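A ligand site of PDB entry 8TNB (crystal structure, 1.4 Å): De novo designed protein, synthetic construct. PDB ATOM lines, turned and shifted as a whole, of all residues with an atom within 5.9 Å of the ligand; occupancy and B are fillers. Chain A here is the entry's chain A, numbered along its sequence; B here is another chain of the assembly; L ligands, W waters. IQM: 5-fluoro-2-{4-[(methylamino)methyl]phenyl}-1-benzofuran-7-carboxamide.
Water W1 bridges the backbone carbonyl oxygen (O) of Phe 123 and a nitrogen (N19) of the ligand.
NE2 of Gln 54 lies within hydrogen-bond range of O20 of the ligand, 2.9 Å away.
The side-chain carboxylate of Asp 29 is in salt-bridge range of a nitrogen (N02) of the ligand.
The side-chain carboxylate (OD1) of Asp 58 is in hydrogen-bond range of the side-chain amide nitrogen (NE2) of Gln 54, at 3.1 Å.
NZ of Lys 33 of chain B lies within salt-bridge range of OD2 of Asp 29 (3.2 Å).
The backbone carbonyl oxygen of Leu 24 sits at hydrogen-bond distance from the side-chain hydroxyl of Thr 28 (2.8 Å).
Residues that only touch the ligand: Ile 21 (3.4 Å), Leu 24 (3.4 Å), Ala 25 (3.6 Å), Thr 28 (3.8 Å), Glu 32 (3.4 Å), Val 57 (3.6 Å), Leu 90 (3.6 Å), Val 94 (3.5 Å), Ala 97 (3.9 Å), Val 124 (3.7 Å), Gly 127 (3.5 Å), Ala 130 (3.3 Å), Asp 131 (3.6 Å) and Phe 134 (3.4 Å).
Hydrophobic or aromatic side chains within 4 Å of the ligand: Ile 21, Leu 24, Ala 25, Val 57, Leu 90, Val 94, Ala 97, Val 124, Ala 130 and Phe 134.
16 residues have an atom within 4 Å of the ligand: Ile 21, Leu 24, Ala 25, Thr 28, Asp 29, Glu 32, Gln 54, Val 57, Leu 90, Val 94, Ala 97, Val 124, Gly 127, Ala 130, Asp 131 and Phe 134.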
ATOM      1  N   TRP A  18      21.911  18.775  19.549  1.00  0.00           N
ATOM      2  CA  TRP A  18      22.751  19.975  19.630  1.00  0.00           C
ATOM      3  C   TRP A  18      24.190  19.628  20.042  1.00  0.00           C
ATOM      4  O   TRP A  18      25.159  20.190  19.494  1.00  0.00           O
ATOM      5  CB  TRP A  18      22.132  21.008  20.556  1.00  0.00           C
ATOM      6  CG  TRP A  18      22.995  22.235  20.538  1.00  0.00           C
ATOM      7  CD1 TRP A  18      23.729  22.731  21.565  1.00  0.00           C
ATOM      8  CD2 TRP A  18      23.272  23.054  19.390  1.00  0.00           C
ATOM      9  NE1 TRP A  18      24.416  23.858  21.145  1.00  0.00           N
ATOM     10  CE2 TRP A  18      24.168  24.054  19.812  1.00  0.00           C
ATOM     11  CE3 TRP A  18      22.846  23.041  18.052  1.00  0.00           C
ATOM     12  CZ2 TRP A  18      24.638  25.055  18.947  1.00  0.00           C
ATOM     13  CZ3 TRP A  18      23.315  24.031  17.195  1.00  0.00           C
ATOM     14  CH2 TRP A  18      24.198  25.020  17.650  1.00  0.00           C
ATOM     15  N   ILE A  21      25.849  18.157  17.047  1.00  0.00           N
ATOM     16  CA  ILE A  21      26.152  19.185  16.068  1.00  0.00           C
ATOM     17  C   ILE A  21      27.421  19.929  16.473  1.00  0.00           C
ATOM     18  O   ILE A  21      28.277  20.207  15.617  1.00  0.00           O
ATOM     19  CB  ILE A  21      24.963  20.117  15.942  1.00  0.00           C
ATOM     20  CG1 ILE A  21      23.818  19.406  15.226  1.00  0.00           C
ATOM     21  CG2 ILE A  21      25.326  21.434  15.177  1.00  0.00           C
ATOM     22  CD1 ILE A  21      22.477  19.963  15.504  1.00  0.00           C
ATOM     23  N   LEU A  24      30.187  17.678  15.423  1.00  0.00           N
ATOM     24  CA  LEU A  24      30.304  17.728  13.973  1.00  0.00           C
ATOM     25  C   LEU A  24      30.989  18.987  13.507  1.00  0.00           C
ATOM     26  O   LEU A  24      31.854  18.923  12.607  1.00  0.00           O
ATOM     27  CB  LEU A  24      28.923  17.620  13.339  1.00  0.00           C
ATOM     28  CG  LEU A  24      28.914  17.685  11.813  1.00  0.00           C
ATOM     29  CD1 LEU A  24      29.716  16.581  11.182  1.00  0.00           C
ATOM     30  CD2 LEU A  24      27.426  17.654  11.362  1.00  0.00           C
ATOM     31  N   ALA A  25      30.670  20.113  14.143  1.00  0.00           N
ATOM     32  CA  ALA A  25      31.340  21.371  13.806  1.00  0.00           C
ATOM     33  C   ALA A  25      32.841  21.321  14.117  1.00  0.00           C
ATOM     34  O   ALA A  25      33.655  21.741  13.313  1.00  0.00           O
ATOM     35  CB  ALA A  25      30.717  22.496  14.590  1.00  0.00           C
ATOM     36  N   SER A  26      33.218  20.764  15.255  1.00  0.00           N
ATOM     37  CA  SER A  26      34.617  20.714  15.612  1.00  0.00           C
ATOM     38  C   SER A  26      35.363  19.794  14.656  1.00  0.00           C
ATOM     39  O   SER A  26      36.461  20.092  14.193  1.00  0.00           O
ATOM     40  CB  SER A  26      34.766  20.294  17.067  1.00  0.00           C
ATOM     41  OG  SER A  26      36.060  19.880  17.387  1.00  0.00           O
ATOM     42  N   THR A  28      34.549  19.094  11.562  1.00  0.00           N
ATOM     43  CA  THR A  28      34.574  19.726  10.239  1.00  0.00           C
ATOM     44  C   THR A  28      35.659  20.794  10.182  1.00  0.00           C
ATOM     45  O   THR A  28      36.441  20.847   9.224  1.00  0.00           O
ATOM     46  CB  THR A  28      33.218  20.348   9.959  1.00  0.00           C
ATOM     47  OG1 THR A  28      32.197  19.342   9.907  1.00  0.00           O
ATOM     48  CG2 THR A  28      33.235  21.085   8.626  1.00  0.00           C
ATOM     49  N   ASP A  29      35.746  21.597  11.238  1.00  0.00           N
ATOM     50  CA  ASP A  29      36.803  22.614  11.294  1.00  0.00           C
ATOM     51  C   ASP A  29      38.173  21.970  11.310  1.00  0.00           C
ATOM     52  O   ASP A  29      39.100  22.457  10.654  1.00  0.00           O
ATOM     53  CB  ASP A  29      36.622  23.467  12.553  1.00  0.00           C
ATOM     54  CG  ASP A  29      35.462  24.441  12.433  1.00  0.00           C
ATOM     55  OD1 ASP A  29      34.957  24.616  11.304  1.00  0.00           O
ATOM     56  OD2 ASP A  29      35.072  25.009  13.485  1.00  0.00           O
ATOM     57  N   GLU A  32      38.960  20.857   7.772  1.00  0.00           N
ATOM     58  CA  GLU A  32      39.373  22.011   6.968  1.00  0.00           C
ATOM     59  C   GLU A  32      40.826  22.371   7.229  1.00  0.00           C
ATOM     60  O   GLU A  32      41.590  22.642   6.288  1.00  0.00           O
ATOM     61  CB  GLU A  32      38.493  23.211   7.303  1.00  0.00           C
ATOM     62  CG  GLU A  32      37.129  23.213   6.675  1.00  0.00           C
ATOM     63  CD  GLU A  32      36.219  24.294   7.232  1.00  0.00           C
ATOM     64  OE1 GLU A  32      36.737  25.264   7.837  1.00  0.00           O
ATOM     65  OE2 GLU A  32      34.987  24.189   7.094  1.00  0.00           O
ATOM     66  N   GLN A  54      27.706  13.017  11.644  1.00  0.00           N
ATOM     67  CA  GLN A  54      26.639  13.336  10.719  1.00  0.00           C
ATOM     68  C   GLN A  54      25.615  12.217  10.688  1.00  0.00           C
ATOM     69  O   GLN A  54      24.423  12.490  10.684  1.00  0.00           O
ATOM     70  CB  GLN A  54      27.216  13.571   9.338  1.00  0.00           C
ATOM     71  CG  GLN A  54      26.172  13.886   8.279  1.00  0.00           C
ATOM     72  CD  GLN A  54      25.548  15.222   8.516  1.00  0.00           C
ATOM     73  OE1 GLN A  54      26.218  16.239   8.488  1.00  0.00           O
ATOM     74  NE2 GLN A  54      24.260  15.266   8.777  1.00  0.00           N
ATOM     75  N   VAL A  57      23.466  12.821  13.691  1.00  0.00           N
ATOM     76  CA  VAL A  57      22.510  13.888  13.428  1.00  0.00           C
ATOM     77  C   VAL A  57      21.359  13.375  12.592  1.00  0.00           C
ATOM     78  O   VAL A  57      20.192  13.703  12.864  1.00  0.00           O
ATOM     79  CB  VAL A  57      23.172  15.117  12.752  1.00  0.00           C
ATOM     80  CG1 VAL A  57      22.114  16.139  12.448  1.00  0.00           C
ATOM     81  CG2 VAL A  57      24.264  15.653  13.686  1.00  0.00           C
ATOM     82  N   ASP A  58      21.658  12.597  11.552  1.00  0.00           N
ATOM     83  CA  ASP A  58      20.638  12.077  10.658  1.00  0.00           C
ATOM     84  C   ASP A  58      19.635  11.266  11.487  1.00  0.00           C
ATOM     85  O   ASP A  58      18.416  11.447  11.351  1.00  0.00           O
ATOM     86  CB  ASP A  58      21.285  11.125   9.654  1.00  0.00           C
ATOM     87  CG  ASP A  58      22.175  11.784   8.606  1.00  0.00           C
ATOM     88  OD1 ASP A  58      22.170  13.007   8.461  1.00  0.00           O
ATOM     89  OD2 ASP A  58      22.952  11.007   7.961  1.00  0.00           O
ATOM     90  N   LEU A  90      14.079  20.086   7.861  1.00  0.00           N
ATOM     91  CA  LEU A  90      15.348  19.835   8.530  1.00  0.00           C
ATOM     92  C   LEU A  90      15.916  18.477   8.155  1.00  0.00           C
ATOM     93  O   LEU A  90      17.099  18.361   7.808  1.00  0.00           O
ATOM     94  CB  LEU A  90      15.159  19.949  10.027  1.00  0.00           C
ATOM     95  CG  LEU A  90      16.367  19.591  10.900  1.00  0.00           C
ATOM     96  CD1 LEU A  90      17.632  20.427  10.628  1.00  0.00           C
ATOM     97  CD2 LEU A  90      15.966  19.672  12.375  1.00  0.00           C
ATOM     98  N   THR A  93      17.302  18.419   4.652  1.00  0.00           N
ATOM     99  CA  THR A  93      18.542  19.170   4.535  1.00  0.00           C
ATOM    100  C   THR A  93      19.694  18.404   5.164  1.00  0.00           C
ATOM    101  O   THR A  93      20.792  18.327   4.589  1.00  0.00           O
ATOM    102  CB  THR A  93      18.369  20.506   5.209  1.00  0.00           C
ATOM    103  OG1 THR A  93      17.228  21.177   4.650  1.00  0.00           O
ATOM    104  CG2 THR A  93      19.577  21.385   5.043  1.00  0.00           C
ATOM    105  N   VAL A  94      19.454  17.811   6.349  1.00  0.00           N
ATOM    106  CA  VAL A  94      20.454  16.981   7.026  1.00  0.00           C
ATOM    107  C   VAL A  94      20.852  15.793   6.166  1.00  0.00           C
ATOM    108  O   VAL A  94      22.035  15.437   6.060  1.00  0.00           O
ATOM    109  CB  VAL A  94      19.884  16.545   8.399  1.00  0.00           C
ATOM    110  CG1 VAL A  94      20.601  15.402   8.973  1.00  0.00           C
ATOM    111  CG2 VAL A  94      19.864  17.744   9.385  1.00  0.00           C
ATOM    112  N   ALA A  97      23.075  17.015   3.460  1.00  0.00           N
ATOM    113  CA  ALA A  97      24.422  17.225   4.000  1.00  0.00           C
ATOM    114  C   ALA A  97      25.154  15.907   4.132  1.00  0.00           C
ATOM    115  O   ALA A  97      26.338  15.784   3.816  1.00  0.00           O
ATOM    116  CB  ALA A  97      24.370  17.924   5.344  1.00  0.00           C
ATOM    117  N   PHE A 123      28.669  20.712   1.624  1.00  0.00           N
ATOM    118  CA  PHE A 123      28.293  20.187   2.951  1.00  0.00           C
ATOM    119  C   PHE A 123      28.280  21.301   3.967  1.00  0.00           C
ATOM    120  O   PHE A 123      27.368  21.384   4.811  1.00  0.00           O
ATOM    121  CB  PHE A 123      29.335  19.124   3.335  1.00  0.00           C
ATOM    122  CG  PHE A 123      29.391  18.805   4.795  1.00  0.00           C
ATOM    123  CD1 PHE A 123      28.363  18.101   5.405  1.00  0.00           C
ATOM    124  CD2 PHE A 123      30.498  19.176   5.563  1.00  0.00           C
ATOM    125  CE1 PHE A 123      28.449  17.819   6.746  1.00  0.00           C
ATOM    126  CE2 PHE A 123      30.560  18.875   6.904  1.00  0.00           C
ATOM    127  CZ  PHE A 123      29.528  18.190   7.490  1.00  0.00           C
ATOM    128  N   VAL A 124      29.294  22.164   3.951  1.00  0.00           N
ATOM    129  CA  VAL A 124      29.317  23.253   4.898  1.00  0.00           C
ATOM    130  C   VAL A 124      28.099  24.152   4.733  1.00  0.00           C
ATOM    131  O   VAL A 124      27.455  24.542   5.705  1.00  0.00           O
ATOM    132  CB  VAL A 124      30.651  24.013   4.776  1.00  0.00           C
ATOM    133  CG1 VAL A 124      30.577  25.287   5.550  1.00  0.00           C
ATOM    134  CG2 VAL A 124      31.787  23.101   5.258  1.00  0.00           C
ATOM    135  N   LEU A 126      25.149  23.354   3.457  1.00  0.00           N
ATOM    136  CA  LEU A 126      23.958  22.654   3.919  1.00  0.00           C
ATOM    137  C   LEU A 126      23.869  22.635   5.430  1.00  0.00           C
ATOM    138  O   LEU A 126      22.778  22.708   6.000  1.00  0.00           O
ATOM    139  CB  LEU A 126      23.969  21.237   3.357  1.00  0.00           C
ATOM    140  CG  LEU A 126      23.659  21.222   1.865  1.00  0.00           C
ATOM    141  CD1 LEU A 126      24.101  19.935   1.245  1.00  0.00           C
ATOM    142  CD2 LEU A 126      22.159  21.428   1.710  1.00  0.00           C
ATOM    143  N   GLY A 127      25.004  22.499   6.112  1.00  0.00           N
ATOM    144  CA  GLY A 127      24.992  22.585   7.560  1.00  0.00           C
ATOM    145  C   GLY A 127      24.442  23.906   8.072  1.00  0.00           C
ATOM    146  O   GLY A 127      23.690  23.951   9.050  1.00  0.00           O
ATOM    147  N   ASN A 128      24.841  25.012   7.446  1.00  0.00           N
ATOM    148  CA  ASN A 128      24.293  26.298   7.863  1.00  0.00           C
ATOM    149  C   ASN A 128      22.800  26.375   7.584  1.00  0.00           C
ATOM    150  O   ASN A 128      22.048  26.903   8.411  1.00  0.00           O
ATOM    151  CB  ASN A 128      25.064  27.447   7.209  1.00  0.00           C
ATOM    152  CG  ASN A 128      26.461  27.605   7.778  1.00  0.00           C
ATOM    153  OD1 ASN A 128      26.661  27.490   8.991  1.00  0.00           O
ATOM    154  ND2 ASN A 128      27.442  27.834   6.917  1.00  0.00           N
ATOM    155  N   ALA A 130      20.807  23.805   7.592  1.00  0.00           N
ATOM    156  CA  ALA A 130      20.186  22.944   8.590  1.00  0.00           C
ATOM    157  C   ALA A 130      20.126  23.648   9.938  1.00  0.00           C
ATOM    158  O   ALA A 130      19.134  23.538  10.660  1.00  0.00           O
ATOM    159  CB  ALA A 130      20.960  21.640   8.690  1.00  0.00           C
ATOM    160  N   ASP A 131      21.162  24.419  10.273  1.00  0.00           N
ATOM    161  CA  ASP A 131      21.182  25.105  11.553  1.00  0.00           C
ATOM    162  C   ASP A 131      20.055  26.123  11.668  1.00  0.00           C
ATOM    163  O   ASP A 131      19.424  26.265  12.736  1.00  0.00           O
ATOM    164  CB  ASP A 131      22.521  25.798  11.707  1.00  0.00           C
ATOM    165  CG  ASP A 131      22.753  26.277  13.113  1.00  0.00           C
ATOM    166  OD1 ASP A 131      22.939  25.408  13.992  1.00  0.00           O
ATOM    167  OD2 ASP A 131      22.703  27.501  13.335  1.00  0.00           O
ATOM    168  N   PHE A 134      17.028  24.058  12.420  1.00  0.00           N
ATOM    169  CA  PHE A 134      17.077  23.550  13.792  1.00  0.00           C
ATOM    170  C   PHE A 134      16.636  24.620  14.787  1.00  0.00           C
ATOM    171  O   PHE A 134      15.830  24.360  15.689  1.00  0.00           O
ATOM    172  CB  PHE A 134      18.513  23.082  14.075  1.00  0.00           C
ATOM    173  CG  PHE A 134      18.655  22.333  15.338  1.00  0.00           C
ATOM    174  CD1 PHE A 134      18.922  23.001  16.526  1.00  0.00           C
ATOM    175  CD2 PHE A 134      18.577  20.945  15.351  1.00  0.00           C
ATOM    176  CE1 PHE A 134      19.065  22.292  17.703  1.00  0.00           C
ATOM    177  CE2 PHE A 134      18.710  20.254  16.539  1.00  0.00           C
ATOM    178  CZ  PHE A 134      18.965  20.920  17.708  1.00  0.00           C
ATOM    179  N   LYS B  33      38.216  28.414  20.125  1.00  0.00           N
ATOM    180  CA  LYS B  33      37.351  29.252  19.292  1.00  0.00           C
ATOM    181  C   LYS B  33      36.148  29.741  20.098  1.00  0.00           C
ATOM    182  O   LYS B  33      35.776  30.911  20.020  1.00  0.00           O
ATOM    183  CB  LYS B  33      36.927  28.428  18.080  1.00  0.00           C
ATOM    184  CG  LYS B  33      35.910  29.087  17.190  1.00  0.00           C
ATOM    185  CD  LYS B  33      35.527  28.196  15.982  1.00  0.00           C
ATOM    186  CE  LYS B  33      34.614  28.943  15.025  1.00  0.00           C
ATOM    187  NZ  LYS B  33      34.491  28.194  13.742  1.00  0.00           N
HETATM  188  C01 IQM L   1      32.085  24.682   8.852  1.00  0.00           C
HETATM  189  C03 IQM L   1      31.837  23.974  11.093  1.00  0.00           C
HETATM  190  C04 IQM L   1      30.361  23.536  11.137  1.00  0.00           C
HETATM  191  C05 IQM L   1      29.437  24.313  11.798  1.00  0.00           C
HETATM  192  C06 IQM L   1      28.111  23.942  11.853  1.00  0.00           C
HETATM  193  C07 IQM L   1      29.960  22.367  10.511  1.00  0.00           C
HETATM  194  C08 IQM L   1      28.623  22.004  10.562  1.00  0.00           C
HETATM  195  C09 IQM L   1      27.703  22.811  11.177  1.00  0.00           C
HETATM  196  C10 IQM L   1      26.278  22.305  11.267  1.00  0.00           C
HETATM  197  C11 IQM L   1      25.279  22.853  12.050  1.00  0.00           C
HETATM  198  C12 IQM L   1      24.123  22.000  11.881  1.00  0.00           C
HETATM  199  C13 IQM L   1      22.811  22.013  12.399  1.00  0.00           C
HETATM  200  C14 IQM L   1      21.970  20.981  12.014  1.00  0.00           C
HETATM  201  C16 IQM L   1      22.384  19.965  11.164  1.00  0.00           C
HETATM  202  C17 IQM L   1      23.670  19.978  10.665  1.00  0.00           C
HETATM  203  C18 IQM L   1      24.097  18.870   9.728  1.00  0.00           C
HETATM  204  C21 IQM L   1      24.555  21.017  11.050  1.00  0.00           C
HETATM  205  F15 IQM L   1      20.693  20.967  12.486  1.00  0.00           F
HETATM  206  N02 IQM L   1      32.007  25.147  10.231  1.00  0.00           N
HETATM  207  N19 IQM L   1      25.310  18.978   8.987  1.00  0.00           N
HETATM  208  O20 IQM L   1      23.386  17.914   9.580  1.00  0.00           O
HETATM  209  O22 IQM L   1      25.857  21.200  10.697  1.00  0.00           O
HETATM  210  O   HOH W   1      27.838  20.886   7.759  1.00  0.00           O
HETATM  211  O   HOH W   2      28.357  24.032   8.162  1.00  0.00           O
